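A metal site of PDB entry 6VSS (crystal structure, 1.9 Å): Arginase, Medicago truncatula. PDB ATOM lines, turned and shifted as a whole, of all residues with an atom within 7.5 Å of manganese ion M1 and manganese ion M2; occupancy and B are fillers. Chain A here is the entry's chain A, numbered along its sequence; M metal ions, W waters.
NE2 of His 160 lies close to OG of Ser 163 (3.3 Å).
NE2 of His 186 is in hydrogen-bond range of OE2 of Glu 285 (3.0 Å).
The backbone NH (N) of Asp 269 lies within hydrogen-bond range of the backbone carbonyl oxygen (O) of Phe 183 (2.9 Å).
OG of Ser 272 lies within hydrogen-bond range of O of Asp 269.
The backbone NH of Phe 204 lies within hydrogen-bond range of the backbone carbonyl oxygen of Asp 188 (3.0 Å).
NE2 of His 160 sits at hydrogen-bond distance from OG of Ser 267, 2.7 Å away.
OD1 of Asp 271 lies close to N of Ala 185 (3.4 Å).
A ring nitrogen (NE2) of His 182 sits close to the side-chain carboxylate of Asp 184.
Four residues have an atom within 4 Å of manganese ion M1: His 160, Asp 184, Asp 188 and Asp 269.
Along chain A the residues within 4 Å of manganese ion M1 span positions 160 to 269.
Four residues have an atom within 4 Å of manganese ion M2: Asp 184, His 186, Asp 269 and Asp 271.
Manganese ion M1 is bound by OD2 of Asp 184, water W2, ND1 of His 160, OD2 of Asp 269 and OD2 of Asp 188.
Manganese ion M1 has five donor atoms within binding distance.
Water W2 binds manganese ion M2 (2.2 Å).
OD2 of Asp 269 is bound to manganese ion M2 (2.2 Å).
The side-chain carboxylate (OD1) of Asp 184 binds manganese ion M2, at 2.2 Å.
Manganese ion M2 is bound by the side-chain carboxylate (OD1) of Asp 271 (2.2 Å).
Manganese ion M2 is bound by OD2 of Asp 271, at 2.3 Å.
Manganese ion M2 is bound by ND1 of His 186, 2.3 Å away.
Water W1 binds manganese ion M2, at 2.7 Å.
Manganese ion M2 has seven donor atoms within binding distance.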
ATOM      1  N   ASP A 159      -9.345 -14.433   6.689  1.00  0.00           N
ATOM      2  CA  ASP A 159      -8.609 -13.573   5.726  1.00  0.00           C
ATOM      3  C   ASP A 159      -7.210 -13.280   6.307  1.00  0.00           C
ATOM      4  O   ASP A 159      -6.946 -13.591   7.523  1.00  0.00           O
ATOM      5  CB  ASP A 159      -9.467 -12.398   5.223  1.00  0.00           C
ATOM      6  CG  ASP A 159      -9.639 -11.243   6.212  1.00  0.00           C
ATOM      7  OD1 ASP A 159      -8.668 -10.992   6.945  1.00  0.00           O
ATOM      8  OD2 ASP A 159     -10.772 -10.653   6.262  1.00  0.00           O
ATOM      9  N   HIS A 160      -6.332 -12.782   5.465  1.00  0.00           N
ATOM     10  CA  HIS A 160      -4.889 -12.571   5.801  1.00  0.00           C
ATOM     11  C   HIS A 160      -4.702 -11.510   6.885  1.00  0.00           C
ATOM     12  O   HIS A 160      -3.568 -11.405   7.419  1.00  0.00           O
ATOM     13  CB  HIS A 160      -4.106 -12.295   4.489  1.00  0.00           C
ATOM     14  CG  HIS A 160      -2.762 -12.939   4.521  1.00  0.00           C
ATOM     15  ND1 HIS A 160      -2.146 -13.356   3.417  1.00  0.00           N
ATOM     16  CD2 HIS A 160      -2.008 -13.314   5.591  1.00  0.00           C
ATOM     17  CE1 HIS A 160      -1.018 -13.972   3.749  1.00  0.00           C
ATOM     18  NE2 HIS A 160      -0.907 -13.962   5.110  1.00  0.00           N
ATOM     19  N   SER A 161      -5.709 -10.714   7.212  1.00  0.00           N
ATOM     20  CA  SER A 161      -5.575  -9.683   8.272  1.00  0.00           C
ATOM     21  C   SER A 161      -5.173 -10.380   9.565  1.00  0.00           C
ATOM     22  O   SER A 161      -4.474  -9.742  10.366  1.00  0.00           O
ATOM     23  CB  SER A 161      -6.818  -8.907   8.517  1.00  0.00           C
ATOM     24  OG  SER A 161      -7.814  -9.714   9.189  1.00  0.00           O
ATOM     25  N   SER A 163      -2.872 -12.608  10.212  1.00  0.00           N
ATOM     26  CA  SER A 163      -1.405 -12.832  10.386  1.00  0.00           C
ATOM     27  C   SER A 163      -0.773 -11.792  11.356  1.00  0.00           C
ATOM     28  O   SER A 163       0.162 -12.121  12.115  1.00  0.00           O
ATOM     29  CB  SER A 163      -0.719 -12.814   9.081  1.00  0.00           C
ATOM     30  OG  SER A 163      -1.067 -14.008   8.400  1.00  0.00           O
ATOM     31  N   HIS A 182       6.457 -16.313   3.393  1.00  0.00           N
ATOM     32  CA  HIS A 182       5.125 -15.781   3.091  1.00  0.00           C
ATOM     33  C   HIS A 182       4.858 -16.126   1.649  1.00  0.00           C
ATOM     34  O   HIS A 182       5.526 -15.565   0.729  1.00  0.00           O
ATOM     35  CB  HIS A 182       5.106 -14.276   3.413  1.00  0.00           C
ATOM     36  CG  HIS A 182       3.896 -13.499   3.033  1.00  0.00           C
ATOM     37  ND1 HIS A 182       3.961 -12.149   2.726  1.00  0.00           N
ATOM     38  CD2 HIS A 182       2.602 -13.865   2.867  1.00  0.00           C
ATOM     39  CE1 HIS A 182       2.769 -11.744   2.388  1.00  0.00           C
ATOM     40  NE2 HIS A 182       1.904 -12.766   2.481  1.00  0.00           N
ATOM     41  N   PHE A 183       3.900 -16.999   1.449  1.00  0.00           N
ATOM     42  CA  PHE A 183       3.413 -17.241   0.088  1.00  0.00           C
ATOM     43  C   PHE A 183       2.154 -16.426  -0.099  1.00  0.00           C
ATOM     44  O   PHE A 183       1.250 -16.542   0.728  1.00  0.00           O
ATOM     45  CB  PHE A 183       3.076 -18.715  -0.138  1.00  0.00           C
ATOM     46  CG  PHE A 183       4.190 -19.670   0.142  1.00  0.00           C
ATOM     47  CD1 PHE A 183       4.407 -20.145   1.439  1.00  0.00           C
ATOM     48  CD2 PHE A 183       4.987 -20.143  -0.869  1.00  0.00           C
ATOM     49  CE1 PHE A 183       5.379 -21.096   1.690  1.00  0.00           C
ATOM     50  CE2 PHE A 183       5.991 -21.061  -0.626  1.00  0.00           C
ATOM     51  CZ  PHE A 183       6.187 -21.540   0.658  1.00  0.00           C
ATOM     52  N   ASP A 184       2.093 -15.701  -1.198  1.00  0.00           N
ATOM     53  CA  ASP A 184       0.916 -14.898  -1.545  1.00  0.00           C
ATOM     54  C   ASP A 184       1.032 -14.447  -2.999  1.00  0.00           C
ATOM     55  O   ASP A 184       2.137 -14.277  -3.443  1.00  0.00           O
ATOM     56  CB  ASP A 184       0.926 -13.605  -0.727  1.00  0.00           C
ATOM     57  CG  ASP A 184      -0.439 -13.098  -0.349  1.00  0.00           C
ATOM     58  OD1 ASP A 184      -1.246 -12.860  -1.271  1.00  0.00           O
ATOM     59  OD2 ASP A 184      -0.638 -12.967   0.852  1.00  0.00           O
ATOM     60  N   ALA A 185      -0.060 -14.139  -3.656  1.00  0.00           N
ATOM     61  CA  ALA A 185      -0.097 -13.379  -4.937  1.00  0.00           C
ATOM     62  C   ALA A 185       0.184 -11.885  -4.646  1.00  0.00           C
ATOM     63  O   ALA A 185       0.463 -11.121  -5.602  1.00  0.00           O
ATOM     64  CB  ALA A 185      -1.458 -13.536  -5.556  1.00  0.00           C
ATOM     65  N   HIS A 186      -0.075 -11.457  -3.411  1.00  0.00           N
ATOM     66  CA  HIS A 186      -0.104 -10.012  -3.028  1.00  0.00           C
ATOM     67  C   HIS A 186       0.885  -9.753  -1.898  1.00  0.00           C
ATOM     68  O   HIS A 186       0.941 -10.479  -0.919  1.00  0.00           O
ATOM     69  CB  HIS A 186      -1.519  -9.564  -2.556  1.00  0.00           C
ATOM     70  CG  HIS A 186      -2.633 -10.092  -3.377  1.00  0.00           C
ATOM     71  ND1 HIS A 186      -3.302 -11.337  -3.069  1.00  0.00           N
ATOM     72  CD2 HIS A 186      -3.170  -9.563  -4.513  1.00  0.00           C
ATOM     73  CE1 HIS A 186      -4.161 -11.542  -4.046  1.00  0.00           C
ATOM     74  NE2 HIS A 186      -4.110 -10.448  -4.960  1.00  0.00           N
ATOM     75  N   PRO A 187       1.647  -8.659  -1.936  1.00  0.00           N
ATOM     76  CA  PRO A 187       2.566  -8.371  -0.835  1.00  0.00           C
ATOM     77  C   PRO A 187       1.901  -8.101   0.511  1.00  0.00           C
ATOM     78  O   PRO A 187       2.565  -8.294   1.533  1.00  0.00           O
ATOM     79  CB  PRO A 187       3.368  -7.159  -1.291  1.00  0.00           C
ATOM     80  CG  PRO A 187       3.117  -7.060  -2.799  1.00  0.00           C
ATOM     81  CD  PRO A 187       1.735  -7.660  -3.013  1.00  0.00           C
ATOM     82  N   ASP A 188       0.650  -7.595   0.526  1.00  0.00           N
ATOM     83  CA  ASP A 188      -0.012  -7.248   1.819  1.00  0.00           C
ATOM     84  C   ASP A 188       0.879  -6.292   2.659  1.00  0.00           C
ATOM     85  O   ASP A 188       0.947  -6.417   3.939  1.00  0.00           O
ATOM     86  CB  ASP A 188      -0.323  -8.530   2.587  1.00  0.00           C
ATOM     87  CG  ASP A 188      -1.374  -9.439   1.945  1.00  0.00           C
ATOM     88  OD1 ASP A 188      -1.979  -9.065   0.850  1.00  0.00           O
ATOM     89  OD2 ASP A 188      -1.577 -10.502   2.546  1.00  0.00           O
ATOM     90  N   HIS A 200      -6.926  -6.939   5.202  1.00  0.00           N
ATOM     91  CA  HIS A 200      -6.149  -8.163   4.820  1.00  0.00           C
ATOM     92  C   HIS A 200      -5.068  -7.807   3.790  1.00  0.00           C
ATOM     93  O   HIS A 200      -4.276  -8.683   3.486  1.00  0.00           O
ATOM     94  CB  HIS A 200      -7.068  -9.285   4.310  1.00  0.00           C
ATOM     95  CG  HIS A 200      -7.665  -9.072   2.958  1.00  0.00           C
ATOM     96  ND1 HIS A 200      -8.159 -10.139   2.193  1.00  0.00           N
ATOM     97  CD2 HIS A 200      -7.844  -7.950   2.223  1.00  0.00           C
ATOM     98  CE1 HIS A 200      -8.640  -9.680   1.057  1.00  0.00           C
ATOM     99  NE2 HIS A 200      -8.463  -8.328   1.045  1.00  0.00           N
ATOM    100  N   ALA A 201      -5.040  -6.572   3.279  1.00  0.00           N
ATOM    101  CA  ALA A 201      -3.964  -6.083   2.397  1.00  0.00           C
ATOM    102  C   ALA A 201      -2.874  -5.274   3.158  1.00  0.00           C
ATOM    103  O   ALA A 201      -1.975  -4.712   2.465  1.00  0.00           O
ATOM    104  CB  ALA A 201      -4.590  -5.259   1.306  1.00  0.00           C
ATOM    105  N   PRO A 203      -1.443  -6.608   6.671  1.00  0.00           N
ATOM    106  CA  PRO A 203      -0.879  -7.221   7.867  1.00  0.00           C
ATOM    107  C   PRO A 203       0.659  -7.208   7.916  1.00  0.00           C
ATOM    108  O   PRO A 203       1.172  -7.146   9.009  1.00  0.00           O
ATOM    109  CB  PRO A 203      -1.425  -8.659   7.847  1.00  0.00           C
ATOM    110  CG  PRO A 203      -1.617  -8.895   6.342  1.00  0.00           C
ATOM    111  CD  PRO A 203      -2.117  -7.580   5.776  1.00  0.00           C
ATOM    112  N   PHE A 204       1.350  -7.232   6.778  1.00  0.00           N
ATOM    113  CA  PHE A 204       2.840  -7.320   6.815  1.00  0.00           C
ATOM    114  C   PHE A 204       3.404  -5.926   7.079  1.00  0.00           C
ATOM    115  O   PHE A 204       4.508  -5.865   7.692  1.00  0.00           O
ATOM    116  CB  PHE A 204       3.407  -8.154   5.646  1.00  0.00           C
ATOM    117  CG  PHE A 204       3.018  -9.611   5.811  1.00  0.00           C
ATOM    118  CD1 PHE A 204       3.759 -10.465   6.602  1.00  0.00           C
ATOM    119  CD2 PHE A 204       1.829 -10.108   5.279  1.00  0.00           C
ATOM    120  CE1 PHE A 204       3.390 -11.796   6.802  1.00  0.00           C
ATOM    121  CE2 PHE A 204       1.434 -11.417   5.533  1.00  0.00           C
ATOM    122  CZ  PHE A 204       2.195 -12.255   6.308  1.00  0.00           C
ATOM    123  N   SER A 267       3.555 -18.255   6.654  1.00  0.00           N
ATOM    124  CA  SER A 267       2.214 -17.789   6.257  1.00  0.00           C
ATOM    125  C   SER A 267       1.932 -18.223   4.819  1.00  0.00           C
ATOM    126  O   SER A 267       2.612 -17.767   3.863  1.00  0.00           O
ATOM    127  CB  SER A 267       2.060 -16.281   6.451  1.00  0.00           C
ATOM    128  OG  SER A 267       0.723 -15.828   6.180  1.00  0.00           O
ATOM    129  N   ILE A 268       0.861 -19.006   4.661  1.00  0.00           N
ATOM    130  CA  ILE A 268       0.449 -19.503   3.339  1.00  0.00           C
ATOM    131  C   ILE A 268      -0.910 -18.902   3.014  1.00  0.00           C
ATOM    132  O   ILE A 268      -1.930 -19.301   3.684  1.00  0.00           O
ATOM    133  CB  ILE A 268       0.450 -21.045   3.351  1.00  0.00           C
ATOM    134  CG1 ILE A 268       1.668 -21.610   4.067  1.00  0.00           C
ATOM    135  CG2 ILE A 268       0.266 -21.516   1.928  1.00  0.00           C
ATOM    136  CD1 ILE A 268       1.855 -23.125   3.957  1.00  0.00           C
ATOM    137  N   ASP A 269      -0.924 -17.991   2.030  1.00  0.00           N
ATOM    138  CA  ASP A 269      -2.162 -17.467   1.384  1.00  0.00           C
ATOM    139  C   ASP A 269      -2.435 -18.384   0.191  1.00  0.00           C
ATOM    140  O   ASP A 269      -1.645 -18.451  -0.695  1.00  0.00           O
ATOM    141  CB  ASP A 269      -2.046 -15.949   1.085  1.00  0.00           C
ATOM    142  CG  ASP A 269      -3.258 -15.201   0.474  1.00  0.00           C
ATOM    143  OD1 ASP A 269      -4.171 -15.905  -0.090  1.00  0.00           O
ATOM    144  OD2 ASP A 269      -3.302 -13.942   0.565  1.00  0.00           O
ATOM    145  N   VAL A 270      -3.543 -19.101   0.237  1.00  0.00           N
ATOM    146  CA  VAL A 270      -3.923 -20.089  -0.801  1.00  0.00           C
ATOM    147  C   VAL A 270      -3.976 -19.354  -2.170  1.00  0.00           C
ATOM    148  O   VAL A 270      -3.713 -20.031  -3.166  1.00  0.00           O
ATOM    149  CB  VAL A 270      -5.242 -20.744  -0.384  1.00  0.00           C
ATOM    150  CG1 VAL A 270      -5.826 -21.630  -1.417  1.00  0.00           C
ATOM    151  CG2 VAL A 270      -5.082 -21.488   0.936  1.00  0.00           C
ATOM    152  N   ASP A 271      -4.184 -18.039  -2.247  1.00  0.00           N
ATOM    153  CA  ASP A 271      -4.267 -17.332  -3.573  1.00  0.00           C
ATOM    154  C   ASP A 271      -2.840 -17.173  -4.203  1.00  0.00           C
ATOM    155  O   ASP A 271      -2.684 -16.749  -5.406  1.00  0.00           O
ATOM    156  CB  ASP A 271      -5.059 -16.038  -3.444  1.00  0.00           C
ATOM    157  CG  ASP A 271      -4.438 -14.804  -2.782  1.00  0.00           C
ATOM    158  OD1 ASP A 271      -3.233 -14.738  -2.617  1.00  0.00           O
ATOM    159  OD2 ASP A 271      -5.186 -13.885  -2.437  1.00  0.00           O
ATOM    160  N   SER A 272      -1.806 -17.526  -3.434  1.00  0.00           N
ATOM    161  CA  SER A 272      -0.451 -17.754  -3.993  1.00  0.00           C
ATOM    162  C   SER A 272      -0.469 -18.801  -5.140  1.00  0.00           C
ATOM    163  O   SER A 272       0.319 -18.680  -6.105  1.00  0.00           O
ATOM    164  CB  SER A 272       0.506 -18.149  -2.870  1.00  0.00           C
ATOM    165  OG  SER A 272       0.323 -19.532  -2.466  1.00  0.00           O
ATOM    166  N   VAL A 281     -10.769 -19.070  -3.563  1.00  0.00           N
ATOM    167  CA  VAL A 281     -10.200 -17.826  -2.962  1.00  0.00           C
ATOM    168  C   VAL A 281     -10.994 -16.605  -3.434  1.00  0.00           C
ATOM    169  O   VAL A 281     -11.736 -16.706  -4.421  1.00  0.00           O
ATOM    170  CB  VAL A 281      -8.701 -17.656  -3.335  1.00  0.00           C
ATOM    171  CG1 VAL A 281      -7.882 -18.819  -2.826  1.00  0.00           C
ATOM    172  CG2 VAL A 281      -8.547 -17.506  -4.858  1.00  0.00           C
ATOM    173  N   HIS A 283      -9.476 -13.688  -4.257  1.00  0.00           N
ATOM    174  CA  HIS A 283      -8.683 -12.880  -5.211  1.00  0.00           C
ATOM    175  C   HIS A 283      -8.014 -13.777  -6.235  1.00  0.00           C
ATOM    176  O   HIS A 283      -6.897 -14.187  -6.019  1.00  0.00           O
ATOM    177  CB  HIS A 283      -7.690 -11.973  -4.504  1.00  0.00           C
ATOM    178  CG  HIS A 283      -8.389 -10.911  -3.723  1.00  0.00           C
ATOM    179  ND1 HIS A 283      -8.859  -9.733  -4.307  1.00  0.00           N
ATOM    180  CD2 HIS A 283      -8.803 -10.902  -2.432  1.00  0.00           C
ATOM    181  CE1 HIS A 283      -9.506  -9.027  -3.402  1.00  0.00           C
ATOM    182  NE2 HIS A 283      -9.490  -9.727  -2.226  1.00  0.00           N
ATOM    183  N   GLU A 285      -5.829 -14.444  -9.172  1.00  0.00           N
ATOM    184  CA  GLU A 285      -4.745 -13.779  -9.910  1.00  0.00           C
ATOM    185  C   GLU A 285      -4.067 -14.766 -10.831  1.00  0.00           C
ATOM    186  O   GLU A 285      -3.215 -15.526 -10.395  1.00  0.00           O
ATOM    187  CB  GLU A 285      -3.769 -13.193  -8.896  1.00  0.00           C
ATOM    188  CG  GLU A 285      -4.418 -12.255  -7.920  1.00  0.00           C
ATOM    189  CD  GLU A 285      -4.631 -10.854  -8.463  1.00  0.00           C
ATOM    190  OE1 GLU A 285      -4.266 -10.596  -9.678  1.00  0.00           O
ATOM    191  OE2 GLU A 285      -5.164 -10.013  -7.685  1.00  0.00           O
ATOM    192  N   VAL A 311      -4.317 -19.344   5.123  1.00  0.00           N
ATOM    193  CA  VAL A 311      -5.342 -18.276   5.090  1.00  0.00           C
ATOM    194  C   VAL A 311      -5.877 -18.129   3.652  1.00  0.00           C
ATOM    195  O   VAL A 311      -5.235 -18.550   2.677  1.00  0.00           O
ATOM    196  CB  VAL A 311      -4.830 -16.912   5.603  1.00  0.00           C
ATOM    197  CG1 VAL A 311      -4.252 -17.010   7.019  1.00  0.00           C
ATOM    198  CG2 VAL A 311      -3.800 -16.325   4.656  1.00  0.00           C
ATOM    199  N   GLU A 312      -7.019 -17.457   3.618  1.00  0.00           N
ATOM    200  CA  GLU A 312      -7.744 -17.000   2.409  1.00  0.00           C
ATOM    201  C   GLU A 312      -8.404 -18.175   1.697  1.00  0.00           C
ATOM    202  O   GLU A 312      -8.849 -17.939   0.561  1.00  0.00           O
ATOM    203  CB  GLU A 312      -6.876 -16.150   1.494  1.00  0.00           C
ATOM    204  CG  GLU A 312      -6.440 -14.812   2.129  1.00  0.00           C
ATOM    205  CD  GLU A 312      -7.443 -13.667   2.042  1.00  0.00           C
ATOM    206  OE1 GLU A 312      -8.430 -13.782   1.205  1.00  0.00           O
ATOM    207  OE2 GLU A 312      -7.266 -12.659   2.752  1.00  0.00           O
HETATM  208 MN    MN M   1      -2.454 -12.244   1.595  1.00  0.00          MN
HETATM  209 MN    MN M   2      -3.459 -12.891  -1.373  1.00  0.00          MN
HETATM  210  O   HOH W   1      -5.554 -11.622  -0.249  1.00  0.00           O
HETATM  211  O   HOH W   2      -2.981 -11.134  -0.157  1.00  0.00           O
